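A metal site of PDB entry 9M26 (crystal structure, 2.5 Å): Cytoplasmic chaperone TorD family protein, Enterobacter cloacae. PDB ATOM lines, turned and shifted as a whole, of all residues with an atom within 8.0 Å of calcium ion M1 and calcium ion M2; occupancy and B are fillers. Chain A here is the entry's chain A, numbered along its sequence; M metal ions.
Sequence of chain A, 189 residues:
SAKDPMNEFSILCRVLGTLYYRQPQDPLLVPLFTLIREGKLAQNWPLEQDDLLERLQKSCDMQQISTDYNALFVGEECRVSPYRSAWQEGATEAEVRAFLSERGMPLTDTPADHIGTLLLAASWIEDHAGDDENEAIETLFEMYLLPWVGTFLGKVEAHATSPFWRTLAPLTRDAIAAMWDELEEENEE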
ATOM      1  N   LYS A   3      18.803 -20.700   8.009  1.00  0.00           N
ATOM      2  CA  LYS A   3      17.882 -20.144   8.983  1.00  0.00           C
ATOM      3  C   LYS A   3      17.290 -21.274   9.826  1.00  0.00           C
ATOM      4  O   LYS A   3      17.052 -22.372   9.330  1.00  0.00           O
ATOM      5  CB  LYS A   3      16.780 -19.342   8.282  1.00  0.00           C
ATOM      6  CG  LYS A   3      16.712 -17.856   8.642  1.00  0.00           C
ATOM      7  CD  LYS A   3      15.778 -17.041   7.712  1.00  0.00           C
ATOM      8  CE  LYS A   3      14.320 -17.018   8.173  1.00  0.00           C
ATOM      9  NZ  LYS A   3      14.093 -16.206   9.404  1.00  0.00           N
ATOM     10  N   ALA A 177       0.414 -21.515   7.281  1.00  0.00           N
ATOM     11  CA  ALA A 177       0.909 -21.281   5.930  1.00  0.00           C
ATOM     12  C   ALA A 177       2.120 -20.366   5.939  1.00  0.00           C
ATOM     13  O   ALA A 177       3.036 -20.529   5.130  1.00  0.00           O
ATOM     14  CB  ALA A 177      -0.205 -20.709   5.050  1.00  0.00           C
ATOM     15  N   ALA A 178       2.137 -19.386   6.843  1.00  0.00           N
ATOM     16  CA  ALA A 178       3.257 -18.463   6.926  1.00  0.00           C
ATOM     17  C   ALA A 178       4.494 -19.154   7.484  1.00  0.00           C
ATOM     18  O   ALA A 178       5.623 -18.886   7.045  1.00  0.00           O
ATOM     19  CB  ALA A 178       2.880 -17.254   7.770  1.00  0.00           C
ATOM     20  N   MET A 179       4.308 -20.047   8.462  1.00  0.00           N
ATOM     21  CA  MET A 179       5.441 -20.810   8.979  1.00  0.00           C
ATOM     22  C   MET A 179       5.990 -21.750   7.932  1.00  0.00           C
ATOM     23  O   MET A 179       7.216 -21.840   7.761  1.00  0.00           O
ATOM     24  CB  MET A 179       5.016 -21.606  10.204  1.00  0.00           C
ATOM     25  CG  MET A 179       4.808 -20.796  11.457  1.00  0.00           C
ATOM     26  SD  MET A 179       4.504 -21.887  12.861  1.00  0.00           S
ATOM     27  CE  MET A 179       3.024 -22.748  12.341  1.00  0.00           C
ATOM     28  N   TRP A 180       5.106 -22.432   7.213  1.00  0.00           N
ATOM     29  CA  TRP A 180       5.522 -23.425   6.221  1.00  0.00           C
ATOM     30  C   TRP A 180       6.346 -22.794   5.103  1.00  0.00           C
ATOM     31  O   TRP A 180       7.330 -23.388   4.641  1.00  0.00           O
ATOM     32  CB  TRP A 180       4.311 -24.155   5.656  1.00  0.00           C
ATOM     33  CG  TRP A 180       4.692 -25.249   4.719  1.00  0.00           C
ATOM     34  CD1 TRP A 180       4.294 -25.404   3.412  1.00  0.00           C
ATOM     35  CD2 TRP A 180       5.605 -26.325   4.980  1.00  0.00           C
ATOM     36  NE1 TRP A 180       4.860 -26.541   2.874  1.00  0.00           N
ATOM     37  CE2 TRP A 180       5.678 -27.121   3.816  1.00  0.00           C
ATOM     38  CE3 TRP A 180       6.347 -26.716   6.105  1.00  0.00           C
ATOM     39  CZ2 TRP A 180       6.453 -28.271   3.744  1.00  0.00           C
ATOM     40  CZ3 TRP A 180       7.138 -27.855   6.021  1.00  0.00           C
ATOM     41  CH2 TRP A 180       7.176 -28.613   4.855  1.00  0.00           C
ATOM     42  N   ASP A 181       5.948 -21.599   4.653  1.00  0.00           N
ATOM     43  CA  ASP A 181       6.730 -20.921   3.623  1.00  0.00           C
ATOM     44  C   ASP A 181       8.152 -20.664   4.091  1.00  0.00           C
ATOM     45  O   ASP A 181       9.107 -20.833   3.318  1.00  0.00           O
ATOM     46  CB  ASP A 181       6.061 -19.597   3.232  1.00  0.00           C
ATOM     47  CG  ASP A 181       6.942 -18.734   2.337  1.00  0.00           C
ATOM     48  OD1 ASP A 181       7.005 -18.979   1.100  1.00  0.00           O
ATOM     49  OD2 ASP A 181       7.583 -17.814   2.891  1.00  0.00           O
ATOM     50  N   GLU A 182       8.330 -20.305   5.358  1.00  0.00           N
ATOM     51  CA  GLU A 182       9.673 -19.986   5.856  1.00  0.00           C
ATOM     52  C   GLU A 182      10.525 -21.251   6.027  1.00  0.00           C
ATOM     53  O   GLU A 182      11.727 -21.244   5.746  1.00  0.00           O
ATOM     54  CB  GLU A 182       9.544 -19.235   7.172  1.00  0.00           C
ATOM     55  CG  GLU A 182      10.468 -18.045   7.294  1.00  0.00           C
ATOM     56  CD  GLU A 182      10.280 -17.055   6.147  1.00  0.00           C
ATOM     57  OE1 GLU A 182      11.286 -16.437   5.741  1.00  0.00           O
ATOM     58  OE2 GLU A 182       9.148 -16.921   5.629  1.00  0.00           O
ATOM     59  N   LEU A 183       9.908 -22.342   6.505  1.00  0.00           N
ATOM     60  CA  LEU A 183      10.594 -23.630   6.618  1.00  0.00           C
ATOM     61  C   LEU A 183      10.966 -24.192   5.250  1.00  0.00           C
ATOM     62  O   LEU A 183      12.096 -24.635   5.029  1.00  0.00           O
ATOM     63  CB  LEU A 183       9.733 -24.624   7.404  1.00  0.00           C
ATOM     64  CG  LEU A 183       9.355 -24.180   8.824  1.00  0.00           C
ATOM     65  CD1 LEU A 183       8.124 -24.921   9.338  1.00  0.00           C
ATOM     66  CD2 LEU A 183      10.521 -24.351   9.768  1.00  0.00           C
ATOM     67  N   GLU A 184      10.000 -24.210   4.319  1.00  0.00           N
ATOM     68  CA  GLU A 184      10.269 -24.757   2.990  1.00  0.00           C
ATOM     69  C   GLU A 184      11.374 -23.985   2.292  1.00  0.00           C
ATOM     70  O   GLU A 184      12.155 -24.588   1.537  1.00  0.00           O
ATOM     71  CB  GLU A 184       9.022 -24.752   2.125  1.00  0.00           C
ATOM     72  CG  GLU A 184       8.238 -26.039   2.164  1.00  0.00           C
ATOM     73  CD  GLU A 184       9.036 -27.262   1.729  1.00  0.00           C
ATOM     74  OE1 GLU A 184       9.792 -27.811   2.555  1.00  0.00           O
ATOM     75  OE2 GLU A 184       8.889 -27.697   0.567  1.00  0.00           O
ATOM     76  N   GLU A 185      11.482 -22.669   2.534  1.00  0.00           N
ATOM     77  CA  GLU A 185      12.532 -21.903   1.886  1.00  0.00           C
ATOM     78  C   GLU A 185      13.909 -22.361   2.352  1.00  0.00           C
ATOM     79  O   GLU A 185      14.889 -22.237   1.617  1.00  0.00           O
ATOM     80  CB  GLU A 185      12.371 -20.406   2.163  1.00  0.00           C
ATOM     81  CG  GLU A 185      11.290 -19.706   1.355  1.00  0.00           C
ATOM     82  CD  GLU A 185      10.855 -18.384   1.979  1.00  0.00           C
ATOM     83  OE1 GLU A 185      11.189 -18.123   3.149  1.00  0.00           O
ATOM     84  OE2 GLU A 185      10.192 -17.586   1.281  1.00  0.00           O
ATOM     85  N   GLU A 186      13.981 -22.929   3.555  1.00  0.00           N
ATOM     86  CA  GLU A 186      15.219 -23.511   4.053  1.00  0.00           C
ATOM     87  C   GLU A 186      15.327 -24.991   3.725  1.00  0.00           C
ATOM     88  O   GLU A 186      16.442 -25.491   3.508  1.00  0.00           O
ATOM     89  CB  GLU A 186      15.316 -23.317   5.575  1.00  0.00           C
ATOM     90  CG  GLU A 186      15.275 -21.848   6.015  1.00  0.00           C
ATOM     91  CD  GLU A 186      16.215 -20.960   5.201  1.00  0.00           C
ATOM     92  OE1 GLU A 186      17.453 -21.107   5.294  1.00  0.00           O
ATOM     93  OE2 GLU A 186      15.708 -20.121   4.432  1.00  0.00           O
HETATM   94 CA    CA M   1       9.121 -15.989   2.966  1.00  0.00          CA
HETATM   95 CA    CA M   2       8.495 -17.593  -0.663  1.00  0.00          CA
HETATM   96 CA    CA M   3      15.809 -19.000  -1.331  1.00  0.00          CA
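Of the 11 residues printed, 3 come within 4 Å of calcium ion M1. The nearest printed residue that does not touch calcium ion M1 is Ala 178 (6.1 Å).
Two residues have an atom within 4 Å of calcium ion M2: Asp 181 and Glu 185.
Calcium ion M1 is bound by OD2 of Asp 181 (2.4 Å), OE2 of Glu 185 (2.6 Å) and OE2 of Glu 182 (2.8 Å). Calcium ion M1 has three donor atoms within binding distance. Slightly farther from calcium ion M1 lies the side-chain carboxylate (OE1) of Glu 185 (3.0 Å).
Calcium ion M2 is bound by the side-chain carboxylate of Glu 185 (2.6 Å) and the side-chain carboxylate of Asp 181 (2.7 Å). Calcium ion M2 has two donor atoms within binding distance.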
